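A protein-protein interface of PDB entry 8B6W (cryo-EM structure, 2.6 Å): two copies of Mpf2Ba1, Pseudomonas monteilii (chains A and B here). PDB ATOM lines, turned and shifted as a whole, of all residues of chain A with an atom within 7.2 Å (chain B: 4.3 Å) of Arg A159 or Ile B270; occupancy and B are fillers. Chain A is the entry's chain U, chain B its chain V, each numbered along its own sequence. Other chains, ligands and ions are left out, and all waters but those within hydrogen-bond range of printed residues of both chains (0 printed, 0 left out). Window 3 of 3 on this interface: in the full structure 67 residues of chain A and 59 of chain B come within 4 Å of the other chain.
Among the printed residues, pairs that only touch across the chains: Ile A17 with Pro B268, Asn A23 with Val B267, Asn A23 with Pro B268, Asn A23 with Thr B269, Gly A25 with Thr B269, Ala A26 with Ile B270, Asp A158 with Thr B269, Asp A158 with Ile B270, Arg A159 with Thr B166, Arg A159 with Ile B270 and Arg A159 with Gln B273.
Of the printed residues of chain B, Asn A23 touches Val B267 (3.9 Å), Pro B268 (3.5 Å) and Thr B269 (3.9 Å). Of chain B, only Thr B166, Ile B270, Met B272 and Gln B273 come within 4 Å of Arg A159. Of the printed residues of chain A, Thr B166 touches Arg A159 (3.5 Å). Printed residues of chain A within 4 Å of Val B267: Asn A23. Of the printed residues of chain A, Pro B268 touches Ile A17 (3.9 Å) and Asn A23 (3.5 Å). Printed residues of chain A within 4 Å of Thr B269: Asn A23, Gly A25 and Asp A158. The nearest residue of chain A that does not touch Ile B270 is Val A27 (4.7 Å).
Along chain B the printed residues that touch a printed residue of chain A span positions 166 to 273. Of the 17 printed residues of chain A, 7 touch a printed residue of chain B. Hydrophobic or aromatic side chains of chain A that line the printed part of chain B: Ile A17 and Ala A26. Among the printed residues, 13 pairs touch across the chains.
OG1 of Thr B166 sits at hydrogen-bond distance from O of Ile B270 (3.0 Å). The indole nitrogen (NE1) of Trp A296 sits at hydrogen-bond distance from the side-chain carboxylate (OD1) of Asp A158. The backbone NH of Thr B166 sits at hydrogen-bond distance from the backbone carbonyl oxygen of Pro B271. The side-chain hydroxyl (OG1) of Thr B166 sits close to the backbone NH (N) of Met B272, 3.4 Å away. N of Val B267 lies within hydrogen-bond range of O of Gly B167, at 3.1 Å. N of Gly B167 sits at hydrogen-bond distance from O of Ile B270, at 3.4 Å.
No position is printed for both chains.
The backbone carbonyl oxygen (O) of Met B272 lies within hydrogen-bond range of the guanidinium group (NH1) of Arg A159 (3.4 Å). OE1 of Gln B273 is in hydrogen-bond range of NH2 of Arg A155 (2.4 Å).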
ATOM      1  N   ILE A  17      11.790   9.041  -7.788  1.00  0.00           N
ATOM      2  CA  ILE A  17      10.733   9.316  -6.824  1.00  0.00           C
ATOM      3  C   ILE A  17      11.175   8.966  -5.408  1.00  0.00           C
ATOM      4  O   ILE A  17      10.912   9.720  -4.465  1.00  0.00           O
ATOM      5  CB  ILE A  17       9.446   8.568  -7.219  1.00  0.00           C
ATOM      6  CG1 ILE A  17       8.330   8.859  -6.218  1.00  0.00           C
ATOM      7  CG2 ILE A  17       9.681   7.081  -7.273  1.00  0.00           C
ATOM      8  CD1 ILE A  17       6.979   8.338  -6.655  1.00  0.00           C
ATOM      9  N   ASN A  23       7.001   0.916  -3.764  1.00  0.00           N
ATOM     10  CA  ASN A  23       6.046   1.984  -4.011  1.00  0.00           C
ATOM     11  C   ASN A  23       6.603   3.022  -4.967  1.00  0.00           C
ATOM     12  O   ASN A  23       5.855   3.861  -5.475  1.00  0.00           O
ATOM     13  CB  ASN A  23       5.646   2.616  -2.691  1.00  0.00           C
ATOM     14  CG  ASN A  23       5.139   1.589  -1.699  1.00  0.00           C
ATOM     15  OD1 ASN A  23       5.902   1.050  -0.900  1.00  0.00           O
ATOM     16  ND2 ASN A  23       3.848   1.286  -1.770  1.00  0.00           N
ATOM     17  N   GLY A  25       7.687   2.798  -8.581  1.00  0.00           N
ATOM     18  CA  GLY A  25       7.669   1.862  -9.694  1.00  0.00           C
ATOM     19  C   GLY A  25       6.315   1.205  -9.887  1.00  0.00           C
ATOM     20  O   GLY A  25       5.618   0.862  -8.926  1.00  0.00           O
ATOM     21  N   ALA A  26       5.940   1.031 -11.154  1.00  0.00           N
ATOM     22  CA  ALA A  26       4.545   0.922 -11.551  1.00  0.00           C
ATOM     23  C   ALA A  26       3.999  -0.497 -11.444  1.00  0.00           C
ATOM     24  O   ALA A  26       3.357  -0.845 -10.451  1.00  0.00           O
ATOM     25  CB  ALA A  26       4.375   1.429 -12.984  1.00  0.00           C
ATOM     26  N   VAL A  27       4.260  -1.322 -12.457  1.00  0.00           N
ATOM     27  CA  VAL A  27       3.607  -2.616 -12.611  1.00  0.00           C
ATOM     28  C   VAL A  27       4.602  -3.650 -13.125  1.00  0.00           C
ATOM     29  O   VAL A  27       5.526  -3.339 -13.878  1.00  0.00           O
ATOM     30  CB  VAL A  27       2.393  -2.505 -13.557  1.00  0.00           C
ATOM     31  CG1 VAL A  27       2.843  -2.120 -14.959  1.00  0.00           C
ATOM     32  CG2 VAL A  27       1.606  -3.803 -13.577  1.00  0.00           C
ATOM     33  N   MET A 138       1.859  -5.671 -22.014  1.00  0.00           N
ATOM     34  CA  MET A 138       2.941  -4.720 -21.800  1.00  0.00           C
ATOM     35  C   MET A 138       3.827  -4.608 -23.033  1.00  0.00           C
ATOM     36  O   MET A 138       4.255  -3.506 -23.396  1.00  0.00           O
ATOM     37  CB  MET A 138       3.776  -5.128 -20.591  1.00  0.00           C
ATOM     38  CG  MET A 138       2.984  -5.301 -19.312  1.00  0.00           C
ATOM     39  SD  MET A 138       1.894  -3.911 -18.943  1.00  0.00           S
ATOM     40  CE  MET A 138       2.985  -2.512 -19.169  1.00  0.00           C
ATOM     41  N   GLN A 141       2.021  -2.599 -25.632  1.00  0.00           N
ATOM     42  CA  GLN A 141       1.990  -1.223 -25.154  1.00  0.00           C
ATOM     43  C   GLN A 141       3.325  -0.530 -25.379  1.00  0.00           C
ATOM     44  O   GLN A 141       3.368   0.654 -25.730  1.00  0.00           O
ATOM     45  CB  GLN A 141       1.629  -1.195 -23.672  1.00  0.00           C
ATOM     46  CG  GLN A 141       1.459   0.205 -23.119  1.00  0.00           C
ATOM     47  CD  GLN A 141       1.205   0.208 -21.632  1.00  0.00           C
ATOM     48  OE1 GLN A 141       1.107  -0.846 -21.005  1.00  0.00           O
ATOM     49  NE2 GLN A 141       1.104   1.396 -21.053  1.00  0.00           N
ATOM     50  N   ILE A 153       5.915   9.648 -25.039  1.00  0.00           N
ATOM     51  CA  ILE A 153       7.062   9.068 -24.348  1.00  0.00           C
ATOM     52  C   ILE A 153       7.092   9.515 -22.895  1.00  0.00           C
ATOM     53  O   ILE A 153       7.302   8.706 -21.985  1.00  0.00           O
ATOM     54  CB  ILE A 153       8.370   9.435 -25.074  1.00  0.00           C
ATOM     55  CG1 ILE A 153       8.281   9.094 -26.563  1.00  0.00           C
ATOM     56  CG2 ILE A 153       9.548   8.718 -24.435  1.00  0.00           C
ATOM     57  CD1 ILE A 153       9.496   9.515 -27.357  1.00  0.00           C
ATOM     58  N   SER A 154       6.875  10.807 -22.646  1.00  0.00           N
ATOM     59  CA  SER A 154       6.917  11.297 -21.274  1.00  0.00           C
ATOM     60  C   SER A 154       5.858  10.611 -20.422  1.00  0.00           C
ATOM     61  O   SER A 154       6.115  10.241 -19.271  1.00  0.00           O
ATOM     62  CB  SER A 154       6.731  12.810 -21.254  1.00  0.00           C
ATOM     63  OG  SER A 154       6.745  13.303 -19.927  1.00  0.00           O
ATOM     64  N   ARG A 155       4.660  10.427 -20.973  1.00  0.00           N
ATOM     65  CA  ARG A 155       3.606   9.710 -20.263  1.00  0.00           C
ATOM     66  C   ARG A 155       3.974   8.252 -20.027  1.00  0.00           C
ATOM     67  O   ARG A 155       3.673   7.696 -18.965  1.00  0.00           O
ATOM     68  CB  ARG A 155       2.297   9.792 -21.041  1.00  0.00           C
ATOM     69  CG  ARG A 155       1.124   9.186 -20.294  1.00  0.00           C
ATOM     70  CD  ARG A 155      -0.191   9.416 -21.005  1.00  0.00           C
ATOM     71  NE  ARG A 155      -1.288   8.739 -20.324  1.00  0.00           N
ATOM     72  CZ  ARG A 155      -1.883   9.186 -19.227  1.00  0.00           C
ATOM     73  NH1 ARG A 155      -1.523  10.325 -18.660  1.00  0.00           N
ATOM     74  NH2 ARG A 155      -2.863   8.469 -18.685  1.00  0.00           N
ATOM     75  N   TYR A 156       4.627   7.618 -20.998  1.00  0.00           N
ATOM     76  CA  TYR A 156       5.066   6.237 -20.822  1.00  0.00           C
ATOM     77  C   TYR A 156       6.025   6.091 -19.649  1.00  0.00           C
ATOM     78  O   TYR A 156       5.839   5.224 -18.789  1.00  0.00           O
ATOM     79  CB  TYR A 156       5.712   5.727 -22.108  1.00  0.00           C
ATOM     80  CG  TYR A 156       5.986   4.246 -22.075  1.00  0.00           C
ATOM     81  CD1 TYR A 156       4.997   3.337 -22.409  1.00  0.00           C
ATOM     82  CD2 TYR A 156       7.220   3.757 -21.686  1.00  0.00           C
ATOM     83  CE1 TYR A 156       5.248   1.986 -22.415  1.00  0.00           C
ATOM     84  CE2 TYR A 156       7.469   2.403 -21.653  1.00  0.00           C
ATOM     85  CZ  TYR A 156       6.482   1.522 -22.030  1.00  0.00           C
ATOM     86  OH  TYR A 156       6.711   0.170 -21.960  1.00  0.00           O
ATOM     87  N   PHE A 157       7.053   6.933 -19.580  1.00  0.00           N
ATOM     88  CA  PHE A 157       7.940   6.886 -18.423  1.00  0.00           C
ATOM     89  C   PHE A 157       7.192   7.202 -17.138  1.00  0.00           C
ATOM     90  O   PHE A 157       7.486   6.628 -16.083  1.00  0.00           O
ATOM     91  CB  PHE A 157       9.096   7.869 -18.594  1.00  0.00           C
ATOM     92  CG  PHE A 157       9.973   7.589 -19.777  1.00  0.00           C
ATOM     93  CD1 PHE A 157      10.180   6.298 -20.221  1.00  0.00           C
ATOM     94  CD2 PHE A 157      10.617   8.624 -20.427  1.00  0.00           C
ATOM     95  CE1 PHE A 157      10.994   6.049 -21.303  1.00  0.00           C
ATOM     96  CE2 PHE A 157      11.431   8.377 -21.507  1.00  0.00           C
ATOM     97  CZ  PHE A 157      11.620   7.090 -21.945  1.00  0.00           C
ATOM     98  N   ASP A 158       6.217   8.104 -17.201  1.00  0.00           N
ATOM     99  CA  ASP A 158       5.383   8.376 -16.035  1.00  0.00           C
ATOM    100  C   ASP A 158       4.547   7.171 -15.628  1.00  0.00           C
ATOM    101  O   ASP A 158       4.463   6.839 -14.442  1.00  0.00           O
ATOM    102  CB  ASP A 158       4.475   9.568 -16.320  1.00  0.00           C
ATOM    103  CG  ASP A 158       5.248  10.850 -16.522  1.00  0.00           C
ATOM    104  OD1 ASP A 158       6.396  10.930 -16.042  1.00  0.00           O
ATOM    105  OD2 ASP A 158       4.712  11.775 -17.167  1.00  0.00           O
ATOM    106  N   ARG A 159       3.922   6.500 -16.591  1.00  0.00           N
ATOM    107  CA  ARG A 159       2.947   5.470 -16.265  1.00  0.00           C
ATOM    108  C   ARG A 159       3.545   4.091 -16.017  1.00  0.00           C
ATOM    109  O   ARG A 159       2.896   3.272 -15.359  1.00  0.00           O
ATOM    110  CB  ARG A 159       1.911   5.361 -17.386  1.00  0.00           C
ATOM    111  CG  ARG A 159       1.048   6.606 -17.571  1.00  0.00           C
ATOM    112  CD  ARG A 159       0.279   6.997 -16.320  1.00  0.00           C
ATOM    113  NE  ARG A 159      -0.637   5.954 -15.878  1.00  0.00           N
ATOM    114  CZ  ARG A 159      -1.376   6.024 -14.780  1.00  0.00           C
ATOM    115  NH1 ARG A 159      -1.350   7.086 -13.995  1.00  0.00           N
ATOM    116  NH2 ARG A 159      -2.166   5.001 -14.466  1.00  0.00           N
ATOM    117  N   VAL A 160       4.743   3.797 -16.521  1.00  0.00           N
ATOM    118  CA  VAL A 160       5.322   2.477 -16.293  1.00  0.00           C
ATOM    119  C   VAL A 160       6.776   2.567 -15.848  1.00  0.00           C
ATOM    120  O   VAL A 160       7.358   1.569 -15.408  1.00  0.00           O
ATOM    121  CB  VAL A 160       5.182   1.607 -17.556  1.00  0.00           C
ATOM    122  CG1 VAL A 160       5.879   2.247 -18.731  1.00  0.00           C
ATOM    123  CG2 VAL A 160       5.719   0.213 -17.303  1.00  0.00           C
ATOM    124  N   GLY A 161       7.374   3.745 -15.943  1.00  0.00           N
ATOM    125  CA  GLY A 161       8.718   3.943 -15.450  1.00  0.00           C
ATOM    126  C   GLY A 161       9.757   3.854 -16.555  1.00  0.00           C
ATOM    127  O   GLY A 161       9.561   3.219 -17.592  1.00  0.00           O
ATOM    128  N   TRP A 296      12.970  13.886 -19.979  1.00  0.00           N
ATOM    129  CA  TRP A 296      12.229  13.350 -18.842  1.00  0.00           C
ATOM    130  C   TRP A 296      13.077  13.290 -17.578  1.00  0.00           C
ATOM    131  O   TRP A 296      12.645  13.743 -16.513  1.00  0.00           O
ATOM    132  CB  TRP A 296      11.697  11.965 -19.197  1.00  0.00           C
ATOM    133  CG  TRP A 296      10.718  11.426 -18.217  1.00  0.00           C
ATOM    134  CD1 TRP A 296       9.383  11.680 -18.172  1.00  0.00           C
ATOM    135  CD2 TRP A 296      10.993  10.522 -17.146  1.00  0.00           C
ATOM    136  NE1 TRP A 296       8.808  10.995 -17.132  1.00  0.00           N
ATOM    137  CE2 TRP A 296       9.777  10.277 -16.486  1.00  0.00           C
ATOM    138  CE3 TRP A 296      12.152   9.900 -16.677  1.00  0.00           C
ATOM    139  CZ2 TRP A 296       9.684   9.435 -15.384  1.00  0.00           C
ATOM    140  CZ3 TRP A 296      12.059   9.065 -15.583  1.00  0.00           C
ATOM    141  CH2 TRP A 296      10.834   8.838 -14.948  1.00  0.00           C
ATOM    142  N   SER B 126      -3.126   0.037 -17.017  1.00  0.00           N
ATOM    143  CA  SER B 126      -3.592   1.063 -17.954  1.00  0.00           C
ATOM    144  C   SER B 126      -3.404   0.665 -19.419  1.00  0.00           C
ATOM    145  O   SER B 126      -3.366   1.524 -20.302  1.00  0.00           O
ATOM    146  CB  SER B 126      -2.892   2.398 -17.690  1.00  0.00           C
ATOM    147  OG  SER B 126      -1.579   2.397 -18.222  1.00  0.00           O
ATOM    148  N   THR B 166      -6.054   3.214  -9.817  1.00  0.00           N
ATOM    149  CA  THR B 166      -5.179   2.253 -10.471  1.00  0.00           C
ATOM    150  C   THR B 166      -3.979   1.870  -9.619  1.00  0.00           C
ATOM    151  O   THR B 166      -3.213   0.990 -10.024  1.00  0.00           O
ATOM    152  CB  THR B 166      -4.672   2.795 -11.815  1.00  0.00           C
ATOM    153  OG1 THR B 166      -3.994   4.036 -11.610  1.00  0.00           O
ATOM    154  CG2 THR B 166      -5.817   2.998 -12.783  1.00  0.00           C
ATOM    155  N   GLY B 167      -3.789   2.496  -8.463  1.00  0.00           N
ATOM    156  CA  GLY B 167      -2.665   2.186  -7.604  1.00  0.00           C
ATOM    157  C   GLY B 167      -2.986   2.523  -6.165  1.00  0.00           C
ATOM    158  O   GLY B 167      -2.928   3.689  -5.774  1.00  0.00           O
ATOM    159  N   VAL B 267      -0.441   4.428  -4.136  1.00  0.00           N
ATOM    160  CA  VAL B 267       0.877   4.197  -4.715  1.00  0.00           C
ATOM    161  C   VAL B 267       1.280   5.440  -5.499  1.00  0.00           C
ATOM    162  O   VAL B 267       0.658   5.745  -6.525  1.00  0.00           O
ATOM    163  CB  VAL B 267       0.878   2.948  -5.608  1.00  0.00           C
ATOM    164  CG1 VAL B 267       2.164   2.858  -6.387  1.00  0.00           C
ATOM    165  CG2 VAL B 267       0.678   1.702  -4.769  1.00  0.00           C
ATOM    166  N   PRO B 268       2.312   6.176  -5.080  1.00  0.00           N
ATOM    167  CA  PRO B 268       2.480   7.550  -5.575  1.00  0.00           C
ATOM    168  C   PRO B 268       2.902   7.632  -7.028  1.00  0.00           C
ATOM    169  O   PRO B 268       2.838   8.721  -7.610  1.00  0.00           O
ATOM    170  CB  PRO B 268       3.562   8.125  -4.653  1.00  0.00           C
ATOM    171  CG  PRO B 268       4.326   6.943  -4.207  1.00  0.00           C
ATOM    172  CD  PRO B 268       3.316   5.849  -4.056  1.00  0.00           C
ATOM    173  N   THR B 269       3.343   6.531  -7.626  1.00  0.00           N
ATOM    174  CA  THR B 269       3.772   6.533  -9.018  1.00  0.00           C
ATOM    175  C   THR B 269       2.610   6.530 -10.008  1.00  0.00           C
ATOM    176  O   THR B 269       2.647   7.300 -10.973  1.00  0.00           O
ATOM    177  CB  THR B 269       4.718   5.350  -9.286  1.00  0.00           C
ATOM    178  OG1 THR B 269       5.098   5.337 -10.667  1.00  0.00           O
ATOM    179  CG2 THR B 269       4.101   4.019  -8.902  1.00  0.00           C
ATOM    180  N   ILE B 270       1.590   5.700  -9.808  1.00  0.00           N
ATOM    181  CA  ILE B 270       0.427   5.697 -10.696  1.00  0.00           C
ATOM    182  C   ILE B 270      -0.856   5.592  -9.879  1.00  0.00           C
ATOM    183  O   ILE B 270      -1.528   4.554  -9.911  1.00  0.00           O
ATOM    184  CB  ILE B 270       0.501   4.546 -11.710  1.00  0.00           C
ATOM    185  CG1 ILE B 270       0.773   3.214 -10.998  1.00  0.00           C
ATOM    186  CG2 ILE B 270       1.567   4.833 -12.748  1.00  0.00           C
ATOM    187  CD1 ILE B 270       0.967   2.051 -11.934  1.00  0.00           C
ATOM    188  N   PRO B 271      -1.245   6.638  -9.152  1.00  0.00           N
ATOM    189  CA  PRO B 271      -2.388   6.495  -8.240  1.00  0.00           C
ATOM    190  C   PRO B 271      -3.722   6.318  -8.946  1.00  0.00           C
ATOM    191  O   PRO B 271      -4.533   5.490  -8.519  1.00  0.00           O
ATOM    192  CB  PRO B 271      -2.340   7.795  -7.428  1.00  0.00           C
ATOM    193  CG  PRO B 271      -1.700   8.767  -8.338  1.00  0.00           C
ATOM    194  CD  PRO B 271      -0.665   7.988  -9.086  1.00  0.00           C
ATOM    195  N   MET B 272      -3.973   7.064 -10.020  1.00  0.00           N
ATOM    196  CA  MET B 272      -5.259   6.991 -10.700  1.00  0.00           C
ATOM    197  C   MET B 272      -5.101   7.401 -12.156  1.00  0.00           C
ATOM    198  O   MET B 272      -4.179   8.135 -12.518  1.00  0.00           O
ATOM    199  CB  MET B 272      -6.289   7.889 -10.009  1.00  0.00           C
ATOM    200  CG  MET B 272      -5.939   9.364 -10.075  1.00  0.00           C
ATOM    201  SD  MET B 272      -7.016  10.397  -9.073  1.00  0.00           S
ATOM    202  CE  MET B 272      -6.516   9.908  -7.429  1.00  0.00           C
ATOM    203  N   GLN B 273      -6.030   6.928 -12.983  1.00  0.00           N
ATOM    204  CA  GLN B 273      -6.028   7.180 -14.414  1.00  0.00           C
ATOM    205  C   GLN B 273      -7.269   7.974 -14.801  1.00  0.00           C
ATOM    206  O   GLN B 273      -8.361   7.740 -14.280  1.00  0.00           O
ATOM    207  CB  GLN B 273      -5.987   5.867 -15.203  1.00  0.00           C
ATOM    208  CG  GLN B 273      -5.888   6.041 -16.708  1.00  0.00           C
ATOM    209  CD  GLN B 273      -4.594   6.687 -17.145  1.00  0.00           C
ATOM    210  OE1 GLN B 273      -4.350   7.860 -16.870  1.00  0.00           O
ATOM    211  NE2 GLN B 273      -3.761   5.927 -17.842  1.00  0.00           N
